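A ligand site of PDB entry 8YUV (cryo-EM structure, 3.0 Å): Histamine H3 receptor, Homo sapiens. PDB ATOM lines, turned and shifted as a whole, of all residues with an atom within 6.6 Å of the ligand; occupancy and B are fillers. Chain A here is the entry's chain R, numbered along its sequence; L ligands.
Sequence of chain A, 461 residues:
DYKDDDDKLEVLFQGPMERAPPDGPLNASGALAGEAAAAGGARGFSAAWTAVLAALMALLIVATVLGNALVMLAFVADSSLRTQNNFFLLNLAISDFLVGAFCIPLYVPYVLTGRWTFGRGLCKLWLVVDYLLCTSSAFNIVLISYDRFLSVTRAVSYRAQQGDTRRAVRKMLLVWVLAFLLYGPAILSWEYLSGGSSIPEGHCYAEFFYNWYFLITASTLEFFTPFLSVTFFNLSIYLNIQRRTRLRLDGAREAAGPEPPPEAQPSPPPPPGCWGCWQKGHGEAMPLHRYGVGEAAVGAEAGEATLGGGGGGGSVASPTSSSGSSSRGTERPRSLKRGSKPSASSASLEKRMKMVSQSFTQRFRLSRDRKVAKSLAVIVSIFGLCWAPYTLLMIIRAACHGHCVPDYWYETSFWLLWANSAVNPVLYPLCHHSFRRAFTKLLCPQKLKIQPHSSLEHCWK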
ATOM      1  N   TRP A 126      -0.929 -11.988  23.775  1.00  0.00           N
ATOM      2  CA  TRP A 126       0.215 -11.980  22.908  1.00  0.00           C
ATOM      3  C   TRP A 126      -0.165 -12.276  21.487  1.00  0.00           C
ATOM      4  O   TRP A 126       0.330 -11.630  20.568  1.00  0.00           O
ATOM      5  CB  TRP A 126       1.252 -12.952  23.398  1.00  0.00           C
ATOM      6  CG  TRP A 126       2.459 -12.942  22.594  1.00  0.00           C
ATOM      7  CD1 TRP A 126       3.489 -12.110  22.741  1.00  0.00           C
ATOM      8  CD2 TRP A 126       2.805 -13.808  21.531  1.00  0.00           C
ATOM      9  NE1 TRP A 126       4.450 -12.390  21.847  1.00  0.00           N
ATOM     10  CE2 TRP A 126       4.047 -13.421  21.087  1.00  0.00           C
ATOM     11  CE3 TRP A 126       2.186 -14.863  20.946  1.00  0.00           C
ATOM     12  CZ2 TRP A 126       4.677 -14.048  20.072  1.00  0.00           C
ATOM     13  CZ3 TRP A 126       2.822 -15.503  19.914  1.00  0.00           C
ATOM     14  CH2 TRP A 126       4.034 -15.099  19.493  1.00  0.00           C
ATOM     15  N   ASP A 130       0.384  -9.692  18.472  1.00  0.00           N
ATOM     16  CA  ASP A 130       1.362 -10.058  17.445  1.00  0.00           C
ATOM     17  C   ASP A 130       0.731 -10.002  16.071  1.00  0.00           C
ATOM     18  O   ASP A 130       1.262  -9.370  15.169  1.00  0.00           O
ATOM     19  CB  ASP A 130       1.911 -11.457  17.691  1.00  0.00           C
ATOM     20  CG  ASP A 130       3.113 -11.767  16.835  1.00  0.00           C
ATOM     21  OD1 ASP A 130       3.845 -10.824  16.477  1.00  0.00           O
ATOM     22  OD2 ASP A 130       3.330 -12.955  16.527  1.00  0.00           O
ATOM     23  N   TYR A 131      -0.402 -10.665  15.915  1.00  0.00           N
ATOM     24  CA  TYR A 131      -1.078 -10.679  14.629  1.00  0.00           C
ATOM     25  C   TYR A 131      -1.562  -9.299  14.210  1.00  0.00           C
ATOM     26  O   TYR A 131      -1.462  -8.941  13.058  1.00  0.00           O
ATOM     27  CB  TYR A 131      -2.191 -11.735  14.608  1.00  0.00           C
ATOM     28  CG  TYR A 131      -1.645 -13.137  14.666  1.00  0.00           C
ATOM     29  CD1 TYR A 131      -0.970 -13.583  15.777  1.00  0.00           C
ATOM     30  CD2 TYR A 131      -1.774 -13.996  13.585  1.00  0.00           C
ATOM     31  CE1 TYR A 131      -0.448 -14.856  15.843  1.00  0.00           C
ATOM     32  CE2 TYR A 131      -1.257 -15.286  13.639  1.00  0.00           C
ATOM     33  CZ  TYR A 131      -0.602 -15.703  14.773  1.00  0.00           C
ATOM     34  OH  TYR A 131      -0.066 -16.972  14.860  1.00  0.00           O
ATOM     35  N   LEU A 132      -2.065  -8.513  15.150  1.00  0.00           N
ATOM     36  CA  LEU A 132      -2.489  -7.151  14.829  1.00  0.00           C
ATOM     37  C   LEU A 132      -1.353  -6.297  14.337  1.00  0.00           C
ATOM     38  O   LEU A 132      -1.518  -5.585  13.352  1.00  0.00           O
ATOM     39  CB  LEU A 132      -3.149  -6.473  16.037  1.00  0.00           C
ATOM     40  CG  LEU A 132      -3.441  -4.984  15.933  1.00  0.00           C
ATOM     41  CD1 LEU A 132      -4.419  -4.689  14.798  1.00  0.00           C
ATOM     42  CD2 LEU A 132      -3.981  -4.454  17.245  1.00  0.00           C
ATOM     43  N   LEU A 133      -0.206  -6.337  15.003  1.00  0.00           N
ATOM     44  CA  LEU A 133       0.871  -5.466  14.609  1.00  0.00           C
ATOM     45  C   LEU A 133       1.500  -5.898  13.319  1.00  0.00           C
ATOM     46  O   LEU A 133       1.811  -5.057  12.463  1.00  0.00           O
ATOM     47  CB  LEU A 133       1.962  -5.467  15.650  1.00  0.00           C
ATOM     48  CG  LEU A 133       1.649  -4.859  16.986  1.00  0.00           C
ATOM     49  CD1 LEU A 133       2.812  -5.128  17.887  1.00  0.00           C
ATOM     50  CD2 LEU A 133       1.424  -3.408  16.872  1.00  0.00           C
ATOM     51  N   CYS A 134       1.694  -7.187  13.125  1.00  0.00           N
ATOM     52  CA  CYS A 134       2.336  -7.623  11.912  1.00  0.00           C
ATOM     53  C   CYS A 134       1.466  -7.352  10.691  1.00  0.00           C
ATOM     54  O   CYS A 134       1.972  -6.875   9.683  1.00  0.00           O
ATOM     55  CB  CYS A 134       2.745  -9.079  12.019  1.00  0.00           C
ATOM     56  SG  CYS A 134       4.095  -9.352  13.188  1.00  0.00           S
ATOM     57  N   THR A 135       0.181  -7.642  10.770  1.00  0.00           N
ATOM     58  CA  THR A 135      -0.727  -7.365   9.650  1.00  0.00           C
ATOM     59  C   THR A 135      -0.815  -5.880   9.375  1.00  0.00           C
ATOM     60  O   THR A 135      -0.834  -5.465   8.225  1.00  0.00           O
ATOM     61  CB  THR A 135      -2.147  -7.904   9.882  1.00  0.00           C
ATOM     62  OG1 THR A 135      -2.091  -9.214  10.440  1.00  0.00           O
ATOM     63  CG2 THR A 135      -2.892  -8.002   8.578  1.00  0.00           C
ATOM     64  N   TYR A 183      -7.707 -10.767  12.027  1.00  0.00           N
ATOM     65  CA  TYR A 183      -7.385 -11.894  12.900  1.00  0.00           C
ATOM     66  C   TYR A 183      -7.882 -11.855  14.343  1.00  0.00           C
ATOM     67  O   TYR A 183      -8.178 -12.902  14.904  1.00  0.00           O
ATOM     68  CB  TYR A 183      -5.891 -12.139  12.965  1.00  0.00           C
ATOM     69  CG  TYR A 183      -5.275 -12.605  11.735  1.00  0.00           C
ATOM     70  CD1 TYR A 183      -5.413 -13.918  11.398  1.00  0.00           C
ATOM     71  CD2 TYR A 183      -4.558 -11.754  10.967  1.00  0.00           C
ATOM     72  CE1 TYR A 183      -4.810 -14.383  10.288  1.00  0.00           C
ATOM     73  CE2 TYR A 183      -3.940 -12.232   9.843  1.00  0.00           C
ATOM     74  CZ  TYR A 183      -4.070 -13.558   9.513  1.00  0.00           C
ATOM     75  OH  TYR A 183      -3.443 -14.049   8.396  1.00  0.00           O
ATOM     76  N   PHE A 209      -4.577 -22.717  12.047  1.00  0.00           N
ATOM     77  CA  PHE A 209      -3.219 -23.195  11.704  1.00  0.00           C
ATOM     78  C   PHE A 209      -3.108 -24.691  11.584  1.00  0.00           C
ATOM     79  O   PHE A 209      -2.031 -25.228  11.332  1.00  0.00           O
ATOM     80  CB  PHE A 209      -2.134 -22.763  12.714  1.00  0.00           C
ATOM     81  CG  PHE A 209      -2.001 -21.283  12.868  1.00  0.00           C
ATOM     82  CD1 PHE A 209      -1.528 -20.566  11.811  1.00  0.00           C
ATOM     83  CD2 PHE A 209      -2.337 -20.587  14.014  1.00  0.00           C
ATOM     84  CE1 PHE A 209      -1.390 -19.235  11.838  1.00  0.00           C
ATOM     85  CE2 PHE A 209      -2.190 -19.211  14.047  1.00  0.00           C
ATOM     86  CZ  PHE A 209      -1.719 -18.558  12.937  1.00  0.00           C
ATOM     87  N   GLU A 222      -4.138 -10.895   3.769  1.00  0.00           N
ATOM     88  CA  GLU A 222      -3.047 -10.244   4.484  1.00  0.00           C
ATOM     89  C   GLU A 222      -1.791 -10.066   3.666  1.00  0.00           C
ATOM     90  O   GLU A 222      -1.071  -9.093   3.844  1.00  0.00           O
ATOM     91  CB  GLU A 222      -2.711 -11.027   5.750  1.00  0.00           C
ATOM     92  CG  GLU A 222      -1.696 -10.297   6.609  1.00  0.00           C
ATOM     93  CD  GLU A 222      -0.971 -11.221   7.553  1.00  0.00           C
ATOM     94  OE1 GLU A 222      -1.099 -12.456   7.417  1.00  0.00           O
ATOM     95  OE2 GLU A 222      -0.261 -10.684   8.422  1.00  0.00           O
ATOM     96  N   TRP A 387       7.919 -11.811   3.827  1.00  0.00           N
ATOM     97  CA  TRP A 387       6.610 -12.371   4.076  1.00  0.00           C
ATOM     98  C   TRP A 387       6.252 -13.682   3.420  1.00  0.00           C
ATOM     99  O   TRP A 387       5.571 -14.514   4.039  1.00  0.00           O
ATOM    100  CB  TRP A 387       5.619 -11.320   3.691  1.00  0.00           C
ATOM    101  CG  TRP A 387       5.539 -10.301   4.678  1.00  0.00           C
ATOM    102  CD1 TRP A 387       6.423  -9.326   4.932  1.00  0.00           C
ATOM    103  CD2 TRP A 387       4.477 -10.118   5.584  1.00  0.00           C
ATOM    104  NE1 TRP A 387       6.016  -8.565   5.955  1.00  0.00           N
ATOM    105  CE2 TRP A 387       4.814  -9.036   6.375  1.00  0.00           C
ATOM    106  CE3 TRP A 387       3.289 -10.773   5.796  1.00  0.00           C
ATOM    107  CZ2 TRP A 387       4.002  -8.602   7.360  1.00  0.00           C
ATOM    108  CZ3 TRP A 387       2.475 -10.330   6.786  1.00  0.00           C
ATOM    109  CH2 TRP A 387       2.822  -9.278   7.550  1.00  0.00           C
ATOM    110  N   TYR A 390       7.073 -17.306   5.324  1.00  0.00           N
ATOM    111  CA  TYR A 390       6.236 -17.678   6.443  1.00  0.00           C
ATOM    112  C   TYR A 390       4.888 -18.078   5.958  1.00  0.00           C
ATOM    113  O   TYR A 390       4.362 -19.111   6.364  1.00  0.00           O
ATOM    114  CB  TYR A 390       6.086 -16.568   7.447  1.00  0.00           C
ATOM    115  CG  TYR A 390       5.317 -17.031   8.610  1.00  0.00           C
ATOM    116  CD1 TYR A 390       5.956 -17.755   9.559  1.00  0.00           C
ATOM    117  CD2 TYR A 390       3.977 -16.778   8.733  1.00  0.00           C
ATOM    118  CE1 TYR A 390       5.284 -18.212  10.639  1.00  0.00           C
ATOM    119  CE2 TYR A 390       3.291 -17.254   9.821  1.00  0.00           C
ATOM    120  CZ  TYR A 390       3.949 -17.964  10.774  1.00  0.00           C
ATOM    121  OH  TYR A 390       3.271 -18.454  11.868  1.00  0.00           O
ATOM    122  N   THR A 391       4.325 -17.269   5.092  1.00  0.00           N
ATOM    123  CA  THR A 391       2.977 -17.500   4.638  1.00  0.00           C
ATOM    124  C   THR A 391       2.891 -18.857   3.996  1.00  0.00           C
ATOM    125  O   THR A 391       1.948 -19.617   4.238  1.00  0.00           O
ATOM    126  CB  THR A 391       2.572 -16.394   3.645  1.00  0.00           C
ATOM    127  OG1 THR A 391       2.630 -15.120   4.300  1.00  0.00           O
ATOM    128  CG2 THR A 391       1.175 -16.624   3.149  1.00  0.00           C
ATOM    129  N   TYR A 410      10.334 -23.750  10.122  1.00  0.00           N
ATOM    130  CA  TYR A 410       9.219 -22.952  10.560  1.00  0.00           C
ATOM    131  C   TYR A 410       9.639 -21.812  11.444  1.00  0.00           C
ATOM    132  O   TYR A 410       9.222 -20.664  11.242  1.00  0.00           O
ATOM    133  CB  TYR A 410       8.172 -23.770  11.271  1.00  0.00           C
ATOM    134  CG  TYR A 410       7.093 -22.898  11.756  1.00  0.00           C
ATOM    135  CD1 TYR A 410       6.155 -22.424  10.858  1.00  0.00           C
ATOM    136  CD2 TYR A 410       7.031 -22.531  13.076  1.00  0.00           C
ATOM    137  CE1 TYR A 410       5.170 -21.588  11.296  1.00  0.00           C
ATOM    138  CE2 TYR A 410       6.042 -21.700  13.521  1.00  0.00           C
ATOM    139  CZ  TYR A 410       5.109 -21.222  12.640  1.00  0.00           C
ATOM    140  OH  TYR A 410       4.117 -20.374  13.094  1.00  0.00           O
ATOM    141  N   SER A 413      11.351 -18.942   9.566  1.00  0.00           N
ATOM    142  CA  SER A 413      10.487 -18.036   8.816  1.00  0.00           C
ATOM    143  C   SER A 413       9.755 -17.091   9.741  1.00  0.00           C
ATOM    144  O   SER A 413       9.525 -15.926   9.385  1.00  0.00           O
ATOM    145  CB  SER A 413       9.505 -18.786   7.983  1.00  0.00           C
ATOM    146  OG  SER A 413      10.137 -19.489   6.959  1.00  0.00           O
ATOM    147  N   PHE A 414       9.373 -17.558  10.902  1.00  0.00           N
ATOM    148  CA  PHE A 414       8.677 -16.707  11.844  1.00  0.00           C
ATOM    149  C   PHE A 414       9.525 -15.492  12.197  1.00  0.00           C
ATOM    150  O   PHE A 414       9.066 -14.335  12.132  1.00  0.00           O
ATOM    151  CB  PHE A 414       8.325 -17.501  13.086  1.00  0.00           C
ATOM    152  CG  PHE A 414       7.723 -16.704  14.118  1.00  0.00           C
ATOM    153  CD1 PHE A 414       6.432 -16.287  14.003  1.00  0.00           C
ATOM    154  CD2 PHE A 414       8.431 -16.375  15.241  1.00  0.00           C
ATOM    155  CE1 PHE A 414       5.876 -15.541  14.996  1.00  0.00           C
ATOM    156  CE2 PHE A 414       7.871 -15.654  16.216  1.00  0.00           C
ATOM    157  CZ  PHE A 414       6.593 -15.233  16.096  1.00  0.00           C
ATOM    158  N   TRP A 415      10.803 -15.680  12.462  1.00  0.00           N
ATOM    159  CA  TRP A 415      11.646 -14.557  12.854  1.00  0.00           C
ATOM    160  C   TRP A 415      11.928 -13.578  11.713  1.00  0.00           C
ATOM    161  O   TRP A 415      12.247 -12.414  11.965  1.00  0.00           O
ATOM    162  CB  TRP A 415      12.915 -15.030  13.533  1.00  0.00           C
ATOM    163  CG  TRP A 415      12.675 -15.495  14.936  1.00  0.00           C
ATOM    164  CD1 TRP A 415      12.354 -16.748  15.334  1.00  0.00           C
ATOM    165  CD2 TRP A 415      12.724 -14.692  16.112  1.00  0.00           C
ATOM    166  NE1 TRP A 415      12.196 -16.784  16.700  1.00  0.00           N
ATOM    167  CE2 TRP A 415      12.419 -15.534  17.205  1.00  0.00           C
ATOM    168  CE3 TRP A 415      12.992 -13.341  16.361  1.00  0.00           C
ATOM    169  CZ2 TRP A 415      12.382 -15.076  18.516  1.00  0.00           C
ATOM    170  CZ3 TRP A 415      12.956 -12.892  17.668  1.00  0.00           C
ATOM    171  CH2 TRP A 415      12.653 -13.749  18.728  1.00  0.00           C
ATOM    172  N   LEU A 416      11.821 -14.033  10.471  1.00  0.00           N
ATOM    173  CA  LEU A 416      12.044 -13.162   9.314  1.00  0.00           C
ATOM    174  C   LEU A 416      11.051 -12.010   9.189  1.00  0.00           C
ATOM    175  O   LEU A 416      11.429 -10.898   8.837  1.00  0.00           O
ATOM    176  CB  LEU A 416      12.046 -13.989   8.032  1.00  0.00           C
ATOM    177  CG  LEU A 416      12.492 -13.299   6.737  1.00  0.00           C
ATOM    178  CD1 LEU A 416      13.928 -12.823   6.882  1.00  0.00           C
ATOM    179  CD2 LEU A 416      12.366 -14.269   5.564  1.00  0.00           C
ATOM    180  N   LEU A 417       9.775 -12.258   9.472  1.00  0.00           N
ATOM    181  CA  LEU A 417       8.758 -11.213   9.407  1.00  0.00           C
ATOM    182  C   LEU A 417       9.093 -10.140  10.427  1.00  0.00           C
ATOM    183  O   LEU A 417       8.926  -8.952  10.159  1.00  0.00           O
ATOM    184  CB  LEU A 417       7.376 -11.789   9.680  1.00  0.00           C
ATOM    185  CG  LEU A 417       6.881 -12.892   8.740  1.00  0.00           C
ATOM    186  CD1 LEU A 417       5.540 -13.430   9.214  1.00  0.00           C
ATOM    187  CD2 LEU A 417       6.755 -12.352   7.342  1.00  0.00           C
ATOM    188  N   TRP A 418       9.542 -10.549  11.598  1.00  0.00           N
ATOM    189  CA  TRP A 418       9.936  -9.588  12.633  1.00  0.00           C
ATOM    190  C   TRP A 418      11.121  -8.744  12.178  1.00  0.00           C
ATOM    191  O   TRP A 418      11.206  -7.566  12.510  1.00  0.00           O
ATOM    192  CB  TRP A 418      10.220 -10.317  13.949  1.00  0.00           C
ATOM    193  CG  TRP A 418       8.983 -10.560  14.746  1.00  0.00           C
ATOM    194  CD1 TRP A 418       7.740 -10.055  14.506  1.00  0.00           C
ATOM    195  CD2 TRP A 418       8.871 -11.373  15.920  1.00  0.00           C
ATOM    196  NE1 TRP A 418       6.861 -10.494  15.455  1.00  0.00           N
ATOM    197  CE2 TRP A 418       7.525 -11.303  16.336  1.00  0.00           C
ATOM    198  CE3 TRP A 418       9.759 -12.143  16.664  1.00  0.00           C
ATOM    199  CZ2 TRP A 418       7.060 -11.983  17.456  1.00  0.00           C
ATOM    200  CZ3 TRP A 418       9.298 -12.818  17.776  1.00  0.00           C
ATOM    201  CH2 TRP A 418       7.961 -12.733  18.168  1.00  0.00           C
HETATM  202  N1  LIG L   1       4.496 -12.716  13.419  1.00  0.00           N
HETATM  203  C1  LIG L   1       2.319 -13.617  10.555  1.00  0.00           C
HETATM  204  C2  LIG L   1       1.166 -13.363   9.599  1.00  0.00           C
HETATM  205  C3  LIG L   1       0.361 -11.673  11.232  1.00  0.00           C
HETATM  206  C4  LIG L   1       1.317 -12.214  12.281  1.00  0.00           C
HETATM  207  C5  LIG L   1       1.728 -13.658  11.962  1.00  0.00           C
HETATM  208  C6  LIG L   1       2.525 -14.231  13.116  1.00  0.00           C
HETATM  209  C7  LIG L   1       3.941 -13.845  12.974  1.00  0.00           C
HETATM  210  C8  LIG L   1       4.870 -14.545  12.351  1.00  0.00           C
HETATM  211  C9  LIG L   1       5.799 -12.804  13.062  1.00  0.00           C
HETATM  212  N2  LIG L   1       0.031 -12.684  10.228  1.00  0.00           N
HETATM  213  N3  LIG L   1       6.062 -13.891  12.438  1.00  0.00           N
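Residues that only touch the ligand: Leu 417 (3.3 Å), Trp 418 (3.5 Å), Thr 135 (3.6 Å), Tyr 131 (3.7 Å) and Tyr 390 (3.8 Å). Hydrophobic or aromatic side chains within 4 Å of the ligand: Tyr 131, Tyr 390, Phe 414, Leu 417 and Trp 418. The nearest printed residue that does not touch the ligand is Tyr 183 (4.02 Å).
The side-chain carboxylate (OE2) of Glu 222 lies within salt-bridge range of a nitrogen (N2) of the ligand (2.7 Å). OD2 of Asp 130 is in hydrogen-bond range of N1 of the ligand, at 3.3 Å. The side-chain sulfur (SG) of Cys 134 sits at hydrogen-bond distance from a nitrogen (N1) of the ligand (3.4 Å). A nitrogen (N3) of the ligand lies close to the backbone carbonyl oxygen (O) of Phe 414, 3.1 Å away.
The indole nitrogen of Trp 418 is in hydrogen-bond range of the side-chain sulfur of Cys 134, 3.8 Å away. The side-chain hydroxyl (OG1) of Thr 135 is in hydrogen-bond range of the side-chain carboxylate (OE2) of Glu 222. NE1 of Trp 418 sits at hydrogen-bond distance from OD1 of Asp 130. The side-chain hydroxyl of Thr 135 lies within hydrogen-bond range of the backbone carbonyl oxygen of Tyr 131 (2.7 Å). The side-chain carboxylate of Glu 222 sits at hydrogen-bond distance from the side-chain hydroxyl of Tyr 183, at 3.0 Å. The backbone carbonyl oxygen of Asp 130 is in hydrogen-bond range of the side-chain sulfur of Cys 134 (3.5 Å). OH of Tyr 390 sits at hydrogen-bond distance from OH of Tyr 410, at 2.4 Å.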
